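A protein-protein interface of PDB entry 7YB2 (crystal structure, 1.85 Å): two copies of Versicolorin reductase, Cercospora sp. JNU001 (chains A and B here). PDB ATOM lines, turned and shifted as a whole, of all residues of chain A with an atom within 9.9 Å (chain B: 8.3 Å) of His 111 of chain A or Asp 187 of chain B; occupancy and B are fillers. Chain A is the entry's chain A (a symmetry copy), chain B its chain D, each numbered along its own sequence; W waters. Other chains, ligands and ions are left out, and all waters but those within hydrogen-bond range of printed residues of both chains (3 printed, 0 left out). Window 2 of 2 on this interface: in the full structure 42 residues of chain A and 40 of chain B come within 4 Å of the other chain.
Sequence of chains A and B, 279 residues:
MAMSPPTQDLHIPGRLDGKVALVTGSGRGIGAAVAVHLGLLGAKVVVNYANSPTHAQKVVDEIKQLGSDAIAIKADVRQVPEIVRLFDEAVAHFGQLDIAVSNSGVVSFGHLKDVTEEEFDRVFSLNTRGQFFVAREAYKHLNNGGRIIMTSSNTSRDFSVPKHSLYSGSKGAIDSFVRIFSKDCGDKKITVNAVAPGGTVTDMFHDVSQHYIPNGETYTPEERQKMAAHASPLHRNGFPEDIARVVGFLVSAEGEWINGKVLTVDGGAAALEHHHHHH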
ATOM      1  N   SER A 108       0.810 -11.538  -3.192  1.00  0.00           N
ATOM      2  CA  SER A 108       0.742 -10.326  -2.356  1.00  0.00           C
ATOM      3  C   SER A 108       1.181 -10.686  -0.941  1.00  0.00           C
ATOM      4  O   SER A 108       0.825 -11.765  -0.468  1.00  0.00           O
ATOM      5  CB  SER A 108      -0.656  -9.789  -2.381  1.00  0.00           C
ATOM      6  OG  SER A 108      -0.719  -8.618  -1.600  1.00  0.00           O
ATOM      7  N   PHE A 109       1.904  -9.790  -0.278  1.00  0.00           N
ATOM      8  CA  PHE A 109       2.258  -9.894   1.155  1.00  0.00           C
ATOM      9  C   PHE A 109       1.948  -8.552   1.805  1.00  0.00           C
ATOM     10  O   PHE A 109       2.208  -7.485   1.209  1.00  0.00           O
ATOM     11  CB  PHE A 109       3.724 -10.281   1.366  1.00  0.00           C
ATOM     12  CG  PHE A 109       3.913 -11.774   1.446  1.00  0.00           C
ATOM     13  CD1 PHE A 109       3.798 -12.453   2.658  1.00  0.00           C
ATOM     14  CD2 PHE A 109       4.045 -12.516   0.278  1.00  0.00           C
ATOM     15  CE1 PHE A 109       3.923 -13.836   2.709  1.00  0.00           C
ATOM     16  CE2 PHE A 109       4.177 -13.901   0.328  1.00  0.00           C
ATOM     17  CZ  PHE A 109       4.127 -14.557   1.548  1.00  0.00           C
ATOM     18  N   GLY A 110       1.462  -8.614   3.033  1.00  0.00           N
ATOM     19  CA  GLY A 110       1.182  -7.402   3.823  1.00  0.00           C
ATOM     20  C   GLY A 110       0.335  -7.777   4.997  1.00  0.00           C
ATOM     21  O   GLY A 110      -0.546  -8.640   4.844  1.00  0.00           O
ATOM     22  N   HIS A 111       0.658  -7.230   6.157  1.00  0.00           N
ATOM     23  CA  HIS A 111      -0.170  -7.377   7.363  1.00  0.00           C
ATOM     24  C   HIS A 111      -1.567  -6.853   7.039  1.00  0.00           C
ATOM     25  O   HIS A 111      -1.692  -5.884   6.299  1.00  0.00           O
ATOM     26  CB  HIS A 111       0.490  -6.608   8.512  1.00  0.00           C
ATOM     27  CG  HIS A 111      -0.100  -6.838   9.847  1.00  0.00           C
ATOM     28  ND1 HIS A 111      -1.372  -6.375  10.171  1.00  0.00           N
ATOM     29  CD2 HIS A 111       0.459  -7.340  10.968  1.00  0.00           C
ATOM     30  CE1 HIS A 111      -1.592  -6.682  11.437  1.00  0.00           C
ATOM     31  NE2 HIS A 111      -0.490  -7.257  11.949  1.00  0.00           N
ATOM     32  N   LEU A 112      -2.579  -7.506   7.590  1.00  0.00           N
ATOM     33  CA  LEU A 112      -3.969  -7.106   7.439  1.00  0.00           C
ATOM     34  C   LEU A 112      -4.073  -5.578   7.615  1.00  0.00           C
ATOM     35  O   LEU A 112      -4.750  -4.962   6.814  1.00  0.00           O
ATOM     36  CB  LEU A 112      -4.777  -7.865   8.492  1.00  0.00           C
ATOM     37  CG  LEU A 112      -6.181  -7.338   8.746  1.00  0.00           C
ATOM     38  CD1 LEU A 112      -7.050  -7.384   7.490  1.00  0.00           C
ATOM     39  CD2 LEU A 112      -6.835  -8.059   9.896  1.00  0.00           C
ATOM     40  N   LYS A 113      -3.456  -4.992   8.642  1.00  0.00           N
ATOM     41  CA  LYS A 113      -3.639  -3.537   8.917  1.00  0.00           C
ATOM     42  C   LYS A 113      -3.227  -2.672   7.713  1.00  0.00           C
ATOM     43  O   LYS A 113      -3.726  -1.517   7.630  1.00  0.00           O
ATOM     44  CB  LYS A 113      -2.875  -3.159  10.191  1.00  0.00           C
ATOM     45  CG  LYS A 113      -1.374  -2.963  10.009  1.00  0.00           C
ATOM     46  CD  LYS A 113      -0.621  -3.006  11.329  1.00  0.00           C
ATOM     47  CE  LYS A 113       0.551  -2.052  11.385  1.00  0.00           C
ATOM     48  NZ  LYS A 113       1.668  -2.494  10.527  1.00  0.00           N
ATOM     49  N   ASP A 114      -2.384  -3.183   6.793  1.00  0.00           N
ATOM     50  CA  ASP A 114      -1.723  -2.381   5.731  1.00  0.00           C
ATOM     51  C   ASP A 114      -2.406  -2.608   4.377  1.00  0.00           C
ATOM     52  O   ASP A 114      -2.046  -1.943   3.440  1.00  0.00           O
ATOM     53  CB  ASP A 114      -0.233  -2.700   5.642  1.00  0.00           C
ATOM     54  CG  ASP A 114       0.549  -2.274   6.879  1.00  0.00           C
ATOM     55  OD1 ASP A 114       0.252  -1.164   7.427  1.00  0.00           O
ATOM     56  OD2 ASP A 114       1.369  -3.095   7.353  1.00  0.00           O
ATOM     57  N   VAL A 115      -3.348  -3.543   4.275  1.00  0.00           N
ATOM     58  CA  VAL A 115      -3.937  -3.923   2.974  1.00  0.00           C
ATOM     59  C   VAL A 115      -4.920  -2.835   2.546  1.00  0.00           C
ATOM     60  O   VAL A 115      -5.889  -2.566   3.283  1.00  0.00           O
ATOM     61  CB  VAL A 115      -4.600  -5.321   3.018  1.00  0.00           C
ATOM     62  CG1 VAL A 115      -5.290  -5.659   1.698  1.00  0.00           C
ATOM     63  CG2 VAL A 115      -3.589  -6.419   3.358  1.00  0.00           C
ATOM     64  N   THR A 116      -4.726  -2.325   1.336  1.00  0.00           N
ATOM     65  CA  THR A 116      -5.583  -1.274   0.738  1.00  0.00           C
ATOM     66  C   THR A 116      -6.729  -1.899  -0.049  1.00  0.00           C
ATOM     67  O   THR A 116      -6.625  -3.079  -0.476  1.00  0.00           O
ATOM     68  CB  THR A 116      -4.742  -0.345  -0.139  1.00  0.00           C
ATOM     69  OG1 THR A 116      -4.156  -1.067  -1.230  1.00  0.00           O
ATOM     70  CG2 THR A 116      -3.687   0.320   0.702  1.00  0.00           C
ATOM     71  N   GLU A 119      -5.105  -2.911  -3.380  1.00  0.00           N
ATOM     72  CA  GLU A 119      -4.325  -4.181  -3.311  1.00  0.00           C
ATOM     73  C   GLU A 119      -5.298  -5.370  -3.237  1.00  0.00           C
ATOM     74  O   GLU A 119      -5.065  -6.339  -3.943  1.00  0.00           O
ATOM     75  CB  GLU A 119      -3.349  -4.157  -2.140  1.00  0.00           C
ATOM     76  CG  GLU A 119      -2.395  -5.348  -2.137  1.00  0.00           C
ATOM     77  CD  GLU A 119      -1.559  -5.562  -3.390  1.00  0.00           C
ATOM     78  OE1 GLU A 119      -1.585  -4.700  -4.300  1.00  0.00           O
ATOM     79  OE2 GLU A 119      -0.889  -6.607  -3.464  1.00  0.00           O
ATOM     80  N   VAL A 161       0.907 -18.646   6.674  1.00  0.00           N
ATOM     81  CA  VAL A 161       2.114 -17.771   6.652  1.00  0.00           C
ATOM     82  C   VAL A 161       1.670 -16.396   7.140  1.00  0.00           C
ATOM     83  O   VAL A 161       0.681 -15.888   6.640  1.00  0.00           O
ATOM     84  CB  VAL A 161       2.658 -17.735   5.211  1.00  0.00           C
ATOM     85  CG1 VAL A 161       3.946 -16.933   5.110  1.00  0.00           C
ATOM     86  CG2 VAL A 161       2.816 -19.155   4.649  1.00  0.00           C
ATOM     87  N   PRO A 162       2.350 -15.749   8.104  1.00  0.00           N
ATOM     88  CA  PRO A 162       2.001 -14.376   8.486  1.00  0.00           C
ATOM     89  C   PRO A 162       2.031 -13.406   7.302  1.00  0.00           C
ATOM     90  O   PRO A 162       2.837 -13.584   6.414  1.00  0.00           O
ATOM     91  CB  PRO A 162       3.112 -13.914   9.463  1.00  0.00           C
ATOM     92  CG  PRO A 162       3.810 -15.190   9.860  1.00  0.00           C
ATOM     93  CD  PRO A 162       3.515 -16.275   8.834  1.00  0.00           C
ATOM     94  N   LYS A 163       1.108 -12.438   7.274  1.00  0.00           N
ATOM     95  CA  LYS A 163       1.065 -11.338   6.285  1.00  0.00           C
ATOM     96  C   LYS A 163       0.660 -11.868   4.906  1.00  0.00           C
ATOM     97  O   LYS A 163       0.916 -11.192   3.888  1.00  0.00           O
ATOM     98  CB  LYS A 163       2.438 -10.660   6.217  1.00  0.00           C
ATOM     99  CG  LYS A 163       2.846 -10.000   7.523  1.00  0.00           C
ATOM    100  CD  LYS A 163       4.116  -9.177   7.401  1.00  0.00           C
ATOM    101  CE  LYS A 163       4.500  -8.512   8.703  1.00  0.00           C
ATOM    102  NZ  LYS A 163       4.653  -9.514   9.780  1.00  0.00           N
ATOM    103  N   HIS A 164       0.018 -13.038   4.854  1.00  0.00           N
ATOM    104  CA  HIS A 164      -0.334 -13.684   3.573  1.00  0.00           C
ATOM    105  C   HIS A 164      -1.856 -13.802   3.453  1.00  0.00           C
ATOM    106  O   HIS A 164      -2.281 -14.656   2.686  1.00  0.00           O
ATOM    107  CB  HIS A 164       0.393 -15.023   3.488  1.00  0.00           C
ATOM    108  CG  HIS A 164       0.755 -15.446   2.104  1.00  0.00           C
ATOM    109  ND1 HIS A 164       1.054 -14.529   1.078  1.00  0.00           N
ATOM    110  CD2 HIS A 164       0.929 -16.678   1.583  1.00  0.00           C
ATOM    111  CE1 HIS A 164       1.365 -15.215  -0.009  1.00  0.00           C
ATOM    112  NE2 HIS A 164       1.279 -16.531   0.269  1.00  0.00           N
ATOM    113  N   SER A 165      -2.649 -12.981   4.160  1.00  0.00           N
ATOM    114  CA  SER A 165      -4.114 -13.199   4.290  1.00  0.00           C
ATOM    115  C   SER A 165      -4.803 -12.994   2.939  1.00  0.00           C
ATOM    116  O   SER A 165      -5.669 -13.817   2.568  1.00  0.00           O
ATOM    117  CB  SER A 165      -4.735 -12.338   5.363  1.00  0.00           C
ATOM    118  OG  SER A 165      -4.656 -10.960   5.043  1.00  0.00           O
ATOM    119  N   LEU A 166      -4.463 -11.932   2.220  1.00  0.00           N
ATOM    120  CA  LEU A 166      -5.176 -11.541   0.978  1.00  0.00           C
ATOM    121  C   LEU A 166      -4.999 -12.639  -0.083  1.00  0.00           C
ATOM    122  O   LEU A 166      -6.002 -13.150  -0.642  1.00  0.00           O
ATOM    123  CB  LEU A 166      -4.609 -10.200   0.507  1.00  0.00           C
ATOM    124  CG  LEU A 166      -5.210  -9.722  -0.791  1.00  0.00           C
ATOM    125  CD1 LEU A 166      -6.723  -9.559  -0.625  1.00  0.00           C
ATOM    126  CD2 LEU A 166      -4.525  -8.419  -1.258  1.00  0.00           C
ATOM    127  N   TYR A 167      -3.769 -13.100  -0.266  1.00  0.00           N
ATOM    128  CA  TYR A 167      -3.484 -14.134  -1.278  1.00  0.00           C
ATOM    129  C   TYR A 167      -4.140 -15.445  -0.841  1.00  0.00           C
ATOM    130  O   TYR A 167      -4.709 -16.175  -1.697  1.00  0.00           O
ATOM    131  CB  TYR A 167      -1.977 -14.301  -1.416  1.00  0.00           C
ATOM    132  CG  TYR A 167      -1.556 -15.377  -2.369  1.00  0.00           C
ATOM    133  CD1 TYR A 167      -1.545 -15.157  -3.733  1.00  0.00           C
ATOM    134  CD2 TYR A 167      -1.263 -16.642  -1.904  1.00  0.00           C
ATOM    135  CE1 TYR A 167      -1.137 -16.155  -4.610  1.00  0.00           C
ATOM    136  CE2 TYR A 167      -0.828 -17.641  -2.751  1.00  0.00           C
ATOM    137  CZ  TYR A 167      -0.785 -17.398  -4.114  1.00  0.00           C
ATOM    138  OH  TYR A 167      -0.361 -18.365  -4.978  1.00  0.00           O
ATOM    139  N   HIS A 211       9.656 -13.770   2.405  1.00  0.00           N
ATOM    140  CA  HIS A 211       8.471 -13.726   3.302  1.00  0.00           C
ATOM    141  C   HIS A 211       8.122 -15.094   3.883  1.00  0.00           C
ATOM    142  O   HIS A 211       7.266 -15.122   4.760  1.00  0.00           O
ATOM    143  CB  HIS A 211       7.278 -13.079   2.590  1.00  0.00           C
ATOM    144  CG  HIS A 211       7.547 -11.704   2.088  1.00  0.00           C
ATOM    145  ND1 HIS A 211       7.682 -10.636   2.918  1.00  0.00           N
ATOM    146  CD2 HIS A 211       7.707 -11.229   0.845  1.00  0.00           C
ATOM    147  CE1 HIS A 211       7.918  -9.556   2.212  1.00  0.00           C
ATOM    148  NE2 HIS A 211       7.932  -9.894   0.940  1.00  0.00           N
ATOM    149  N   PHE B 132     -13.475  -8.657   4.886  1.00  0.00           N
ATOM    150  CA  PHE B 132     -12.016  -8.441   4.999  1.00  0.00           C
ATOM    151  C   PHE B 132     -11.743  -7.068   5.653  1.00  0.00           C
ATOM    152  O   PHE B 132     -10.892  -6.907   6.554  1.00  0.00           O
ATOM    153  CB  PHE B 132     -11.358  -8.557   3.624  1.00  0.00           C
ATOM    154  CG  PHE B 132      -9.869  -8.386   3.650  1.00  0.00           C
ATOM    155  CD1 PHE B 132      -9.303  -7.113   3.652  1.00  0.00           C
ATOM    156  CD2 PHE B 132      -9.026  -9.482   3.725  1.00  0.00           C
ATOM    157  CE1 PHE B 132      -7.931  -6.942   3.732  1.00  0.00           C
ATOM    158  CE2 PHE B 132      -7.651  -9.307   3.769  1.00  0.00           C
ATOM    159  CZ  PHE B 132      -7.106  -8.047   3.789  1.00  0.00           C
ATOM    160  N   ARG B 136     -10.125  -5.636   9.028  1.00  0.00           N
ATOM    161  CA  ARG B 136      -9.023  -4.642   8.978  1.00  0.00           C
ATOM    162  C   ARG B 136      -9.312  -3.532   9.993  1.00  0.00           C
ATOM    163  O   ARG B 136      -8.448  -3.246  10.853  1.00  0.00           O
ATOM    164  CB  ARG B 136      -8.826  -4.045   7.584  1.00  0.00           C
ATOM    165  CG  ARG B 136      -7.510  -3.278   7.466  1.00  0.00           C
ATOM    166  CD  ARG B 136      -7.420  -2.434   6.231  1.00  0.00           C
ATOM    167  NE  ARG B 136      -8.329  -1.286   6.274  1.00  0.00           N
ATOM    168  CZ  ARG B 136      -8.453  -0.412   5.287  1.00  0.00           C
ATOM    169  NH1 ARG B 136      -7.745  -0.558   4.175  1.00  0.00           N
ATOM    170  NH2 ARG B 136      -9.263   0.628   5.416  1.00  0.00           N
ATOM    171  N   TYR B 139      -9.153  -4.801  13.658  1.00  0.00           N
ATOM    172  CA  TYR B 139      -7.786  -4.915  14.189  1.00  0.00           C
ATOM    173  C   TYR B 139      -7.298  -3.517  14.620  1.00  0.00           C
ATOM    174  O   TYR B 139      -6.663  -3.375  15.683  1.00  0.00           O
ATOM    175  CB  TYR B 139      -6.819  -5.490  13.161  1.00  0.00           C
ATOM    176  CG  TYR B 139      -5.388  -5.400  13.618  1.00  0.00           C
ATOM    177  CD1 TYR B 139      -4.832  -6.354  14.449  1.00  0.00           C
ATOM    178  CD2 TYR B 139      -4.602  -4.323  13.259  1.00  0.00           C
ATOM    179  CE1 TYR B 139      -3.523  -6.253  14.889  1.00  0.00           C
ATOM    180  CE2 TYR B 139      -3.301  -4.195  13.719  1.00  0.00           C
ATOM    181  CZ  TYR B 139      -2.750  -5.180  14.513  1.00  0.00           C
ATOM    182  OH  TYR B 139      -1.452  -5.037  14.934  1.00  0.00           O
ATOM    183  N   LYS B 140      -7.577  -2.520  13.791  1.00  0.00           N
ATOM    184  CA  LYS B 140      -7.049  -1.145  13.977  1.00  0.00           C
ATOM    185  C   LYS B 140      -7.739  -0.446  15.153  1.00  0.00           C
ATOM    186  O   LYS B 140      -7.104   0.412  15.739  1.00  0.00           O
ATOM    187  CB  LYS B 140      -7.188  -0.328  12.693  1.00  0.00           C
ATOM    188  CG  LYS B 140      -6.245  -0.768  11.590  1.00  0.00           C
ATOM    189  CD  LYS B 140      -6.654  -0.314  10.209  1.00  0.00           C
ATOM    190  CE  LYS B 140      -6.467   1.162   9.958  1.00  0.00           C
ATOM    191  NZ  LYS B 140      -7.077   1.557   8.661  1.00  0.00           N
ATOM    192  N   ASN B 144      -6.168  -4.340  22.954  1.00  0.00           N
ATOM    193  CA  ASN B 144      -5.331  -5.547  23.129  1.00  0.00           C
ATOM    194  C   ASN B 144      -6.163  -6.606  23.852  1.00  0.00           C
ATOM    195  O   ASN B 144      -6.961  -6.253  24.736  1.00  0.00           O
ATOM    196  CB  ASN B 144      -4.009  -5.204  23.823  1.00  0.00           C
ATOM    197  CG  ASN B 144      -2.988  -4.582  22.887  1.00  0.00           C
ATOM    198  OD1 ASN B 144      -3.319  -3.943  21.900  1.00  0.00           O
ATOM    199  ND2 ASN B 144      -1.717  -4.728  23.207  1.00  0.00           N
ATOM    200  N   GLY B 145      -6.053  -7.869  23.424  1.00  0.00           N
ATOM    201  CA  GLY B 145      -6.770  -8.979  24.048  1.00  0.00           C
ATOM    202  C   GLY B 145      -8.208  -9.083  23.570  1.00  0.00           C
ATOM    203  O   GLY B 145      -8.957  -9.900  24.130  1.00  0.00           O
ATOM    204  N   ILE B 180      -4.947 -16.861   8.706  1.00  0.00           N
ATOM    205  CA  ILE B 180      -3.790 -15.941   8.570  1.00  0.00           C
ATOM    206  C   ILE B 180      -3.995 -14.728   9.481  1.00  0.00           C
ATOM    207  O   ILE B 180      -3.021 -14.265  10.109  1.00  0.00           O
ATOM    208  CB  ILE B 180      -3.593 -15.487   7.116  1.00  0.00           C
ATOM    209  CG1 ILE B 180      -3.517 -16.647   6.115  1.00  0.00           C
ATOM    210  CG2 ILE B 180      -2.366 -14.580   7.054  1.00  0.00           C
ATOM    211  CD1 ILE B 180      -2.820 -17.882   6.617  1.00  0.00           C
ATOM    212  N   PHE B 181      -5.218 -14.210   9.556  1.00  0.00           N
ATOM    213  CA  PHE B 181      -5.550 -13.077  10.452  1.00  0.00           C
ATOM    214  C   PHE B 181      -5.151 -13.395  11.890  1.00  0.00           C
ATOM    215  O   PHE B 181      -4.709 -12.456  12.607  1.00  0.00           O
ATOM    216  CB  PHE B 181      -7.045 -12.753  10.439  1.00  0.00           C
ATOM    217  CG  PHE B 181      -7.579 -12.075   9.212  1.00  0.00           C
ATOM    218  CD1 PHE B 181      -6.766 -11.650   8.180  1.00  0.00           C
ATOM    219  CD2 PHE B 181      -8.931 -11.832   9.121  1.00  0.00           C
ATOM    220  CE1 PHE B 181      -7.290 -10.995   7.086  1.00  0.00           C
ATOM    221  CE2 PHE B 181      -9.461 -11.179   8.016  1.00  0.00           C
ATOM    222  CZ  PHE B 181      -8.642 -10.758   7.005  1.00  0.00           C
ATOM    223  N   SER B 182      -5.325 -14.634  12.354  1.00  0.00           N
ATOM    224  CA  SER B 182      -4.945 -15.039  13.738  1.00  0.00           C
ATOM    225  C   SER B 182      -3.447 -14.773  13.956  1.00  0.00           C
ATOM    226  O   SER B 182      -3.076 -14.327  15.061  1.00  0.00           O
ATOM    227  CB  SER B 182      -5.327 -16.451  14.091  1.00  0.00           C
ATOM    228  OG  SER B 182      -4.608 -17.414  13.341  1.00  0.00           O
ATOM    229  N   LYS B 183      -2.616 -14.995  12.943  1.00  0.00           N
ATOM    230  CA  LYS B 183      -1.157 -14.705  12.999  1.00  0.00           C
ATOM    231  C   LYS B 183      -0.916 -13.186  13.054  1.00  0.00           C
ATOM    232  O   LYS B 183      -0.242 -12.726  13.979  1.00  0.00           O
ATOM    233  CB  LYS B 183      -0.408 -15.317  11.812  1.00  0.00           C
ATOM    234  CG  LYS B 183      -0.639 -16.807  11.584  1.00  0.00           C
ATOM    235  CD  LYS B 183      -0.282 -17.660  12.773  1.00  0.00           C
ATOM    236  CE  LYS B 183      -0.438 -19.152  12.538  1.00  0.00           C
ATOM    237  NZ  LYS B 183       0.503 -19.626  11.499  1.00  0.00           N
ATOM    238  N   ASP B 184      -1.524 -12.421  12.183  1.00  0.00           N
ATOM    239  CA  ASP B 184      -1.294 -10.958  12.119  1.00  0.00           C
ATOM    240  C   ASP B 184      -1.806 -10.308  13.410  1.00  0.00           C
ATOM    241  O   ASP B 184      -1.098  -9.434  13.934  1.00  0.00           O
ATOM    242  CB  ASP B 184      -1.984 -10.330  10.918  1.00  0.00           C
ATOM    243  CG  ASP B 184      -1.377 -10.680   9.577  1.00  0.00           C
ATOM    244  OD1 ASP B 184      -0.365 -11.377   9.561  1.00  0.00           O
ATOM    245  OD2 ASP B 184      -1.946 -10.260   8.576  1.00  0.00           O
ATOM    246  N   CYS B 185      -2.993 -10.712  13.882  1.00  0.00           N
ATOM    247  CA  CYS B 185      -3.715 -10.055  15.001  1.00  0.00           C
ATOM    248  C   CYS B 185      -3.112 -10.472  16.357  1.00  0.00           C
ATOM    249  O   CYS B 185      -3.407  -9.798  17.361  1.00  0.00           O
ATOM    250  CB  CYS B 185      -5.218 -10.310  14.927  1.00  0.00           C
ATOM    251  SG  CYS B 185      -5.996  -9.611  13.459  1.00  0.00           S
ATOM    252  N   GLY B 186      -2.228 -11.477  16.365  1.00  0.00           N
ATOM    253  CA  GLY B 186      -1.447 -11.883  17.547  1.00  0.00           C
ATOM    254  C   GLY B 186      -0.600 -10.754  18.121  1.00  0.00           C
ATOM    255  O   GLY B 186      -0.374 -10.766  19.333  1.00  0.00           O
ATOM    256  N   ASP B 187      -0.195  -9.777  17.325  1.00  0.00           N
ATOM    257  CA  ASP B 187       0.694  -8.696  17.855  1.00  0.00           C
ATOM    258  C   ASP B 187      -0.112  -7.731  18.762  1.00  0.00           C
ATOM    259  O   ASP B 187       0.554  -6.981  19.495  1.00  0.00           O
ATOM    260  CB  ASP B 187       1.556  -8.116  16.738  1.00  0.00           C
ATOM    261  CG  ASP B 187       0.777  -7.395  15.667  1.00  0.00           C
ATOM    262  OD1 ASP B 187      -0.320  -6.908  16.014  1.00  0.00           O
ATOM    263  OD2 ASP B 187       1.264  -7.365  14.485  1.00  0.00           O
ATOM    264  N   LYS B 188      -1.462  -7.833  18.824  1.00  0.00           N
ATOM    265  CA  LYS B 188      -2.361  -7.149  19.800  1.00  0.00           C
ATOM    266  C   LYS B 188      -3.042  -8.182  20.711  1.00  0.00           C
ATOM    267  O   LYS B 188      -3.981  -7.830  21.454  1.00  0.00           O
ATOM    268  CB  LYS B 188      -3.363  -6.246  19.063  1.00  0.00           C
ATOM    269  CG  LYS B 188      -2.726  -5.022  18.417  1.00  0.00           C
ATOM    270  CD  LYS B 188      -3.675  -4.076  17.722  1.00  0.00           C
ATOM    271  CE  LYS B 188      -4.698  -3.446  18.627  1.00  0.00           C
ATOM    272  NZ  LYS B 188      -5.395  -2.291  17.984  1.00  0.00           N
ATOM    273  N   LYS B 189      -2.587  -9.438  20.672  1.00  0.00           N
ATOM    274  CA  LYS B 189      -3.233 -10.557  21.398  1.00  0.00           C
ATOM    275  C   LYS B 189      -4.737 -10.617  21.082  1.00  0.00           C
ATOM    276  O   LYS B 189      -5.565 -10.979  21.975  1.00  0.00           O
ATOM    277  CB  LYS B 189      -2.909 -10.424  22.878  1.00  0.00           C
ATOM    278  CG  LYS B 189      -1.414 -10.571  23.185  1.00  0.00           C
ATOM    279  CD  LYS B 189      -1.165 -10.704  24.675  1.00  0.00           C
ATOM    280  CE  LYS B 189       0.273 -11.043  25.053  1.00  0.00           C
ATOM    281  NZ  LYS B 189       1.068 -11.483  23.885  1.00  0.00           N
ATOM    282  N   ILE B 190      -5.111 -10.320  19.838  1.00  0.00           N
ATOM    283  CA  ILE B 190      -6.522 -10.491  19.406  1.00  0.00           C
ATOM    284  C   ILE B 190      -6.660 -11.884  18.770  1.00  0.00           C
ATOM    285  O   ILE B 190      -5.853 -12.209  17.908  1.00  0.00           O
ATOM    286  CB  ILE B 190      -6.929  -9.379  18.432  1.00  0.00           C
ATOM    287  CG1 ILE B 190      -6.998  -8.013  19.114  1.00  0.00           C
ATOM    288  CG2 ILE B 190      -8.219  -9.727  17.713  1.00  0.00           C
ATOM    289  CD1 ILE B 190      -6.924  -6.864  18.126  1.00  0.00           C
ATOM    290  N   THR B 191      -7.653 -12.649  19.176  1.00  0.00           N
ATOM    291  CA  THR B 191      -7.972 -13.940  18.507  1.00  0.00           C
ATOM    292  C   THR B 191      -8.903 -13.683  17.331  1.00  0.00           C
ATOM    293  O   THR B 191      -9.697 -12.707  17.357  1.00  0.00           O
ATOM    294  CB  THR B 191      -8.537 -15.000  19.456  1.00  0.00           C
ATOM    295  OG1 THR B 191      -9.845 -14.657  19.920  1.00  0.00           O
ATOM    296  CG2 THR B 191      -7.610 -15.228  20.628  1.00  0.00           C
HETATM  297  O   HOH W   1       2.133 -10.907  10.900  1.00  0.00           O
HETATM  298  O   HOH W   2      -2.180 -10.683   5.966  1.00  0.00           O
HETATM  299  O   HOH W   3      -5.363   0.369   6.636  1.00  0.00           O
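Of chain B, only Tyr 139 (3.6 Å), Asp 184 (3.0 Å) and Asp 187 (3.1 Å) come within 4 Å of His 111 of chain A.
No residue of chain B comes within 4 Å of Gly 110 of chain A.
Asp 184 of chain B touches four residues of chain A.
Cys 185 of chain B touches just one residue of chain A: Leu 112 (3.98 Å).
Printed residues of chain B within 4 Å of Val 115 of chain A: Phe 132 and Arg 136.
Asn 144 of chain B touches none of the printed residues of chain A.
Thr 116 of chain A touches none of the printed residues of chain B.
The nearest residue of chain B that does not touch His 111 of chain A is Cys 185 of chain B (4.7 Å).
The nearest printed residue of chain B that does not touch Pro 162 of chain A is Lys 183 of chain B (4.2 Å).
Among the printed residues, merely in contact across the chains: Leu 112 of chain A with Arg 136 of chain B (3.3 Å), Ser 165 of chain A with Ile 180 of chain B (3.3 Å), Ser 165 of chain A with Phe 181 of chain B (3.3 Å), Val 161 of chain A with Ile 180 of chain B (3.3 Å), Val 115 of chain A with Phe 132 of chain B (3.6 Å), His 164 of chain A with Ile 180 of chain B (3.6 Å), His 111 of chain A with Tyr 139 of chain B (3.6 Å), Leu 112 of chain A with Phe 181 of chain B (3.6 Å), Ser 165 of chain A with Phe 132 of chain B (3.7 Å), Lys 113 of chain A with Tyr 139 of chain B (3.7 Å), Leu 112 of chain A with Phe 132 of chain B (3.8 Å), Pro 162 of chain A with Asp 184 of chain B (3.9 Å) and Leu 112 of chain A with Cys 185 of chain B (3.98 Å).
The backbone carbonyl oxygen (O) of Ser 108 of chain A lies within hydrogen-bond range of a ring nitrogen (ND1) of His 164 of chain A.
OD2 of Asp 114 of chain A is in salt-bridge range of NZ of Lys 113 of chain A (3.2 Å).
Water W3 lies within hydrogen-bond range of the backbone carbonyl oxygen of Lys 113 of chain A (2.7 Å), the side-chain amino group of Lys 140 of chain B (2.9 Å) and the guanidinium group of Arg 136 of chain B (3.4 Å).
Printed residues of chain A that touch a printed residue of chain B: His 111, Leu 112, Lys 113, Val 115, Val 161, Pro 162, Lys 163, His 164 and Ser 165.
Hydrophobic or aromatic side chains of chain A within 4 Å of the printed part of chain B: His 111, Leu 112 and Val 115.
Of the 18 printed residues of chain B, 8 touch a printed residue of chain A.
Hydrophobic or aromatic side chains of chain B that line the printed part of chain A: Phe 132, Tyr 139, Ile 180 and Phe 181.
NH1 of Arg 136 of chain B lies within hydrogen-bond range of O of Val 115 of chain A, 2.9 Å away.
O of Asp 184 of chain B lies within hydrogen-bond range of NE2 of His 111 of chain A, 3.0 Å away.
The backbone NH (N) of Leu 112 of chain A is in hydrogen-bond range of the side-chain carboxylate (OD2) of Asp 184 of chain B (3.0 Å).
The backbone NH of Lys 163 of chain A is in hydrogen-bond range of the side-chain carboxylate of Asp 184 of chain B, at 2.9 Å.
OD2 of Asp 187 of chain B is in hydrogen-bond range of NE2 of His 111 of chain A, 3.1 Å away.
No position is printed for both chains.
Of the 18 pairs that touch across the chains among the printed residues, none has its exchanged pair printed and touching as well.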
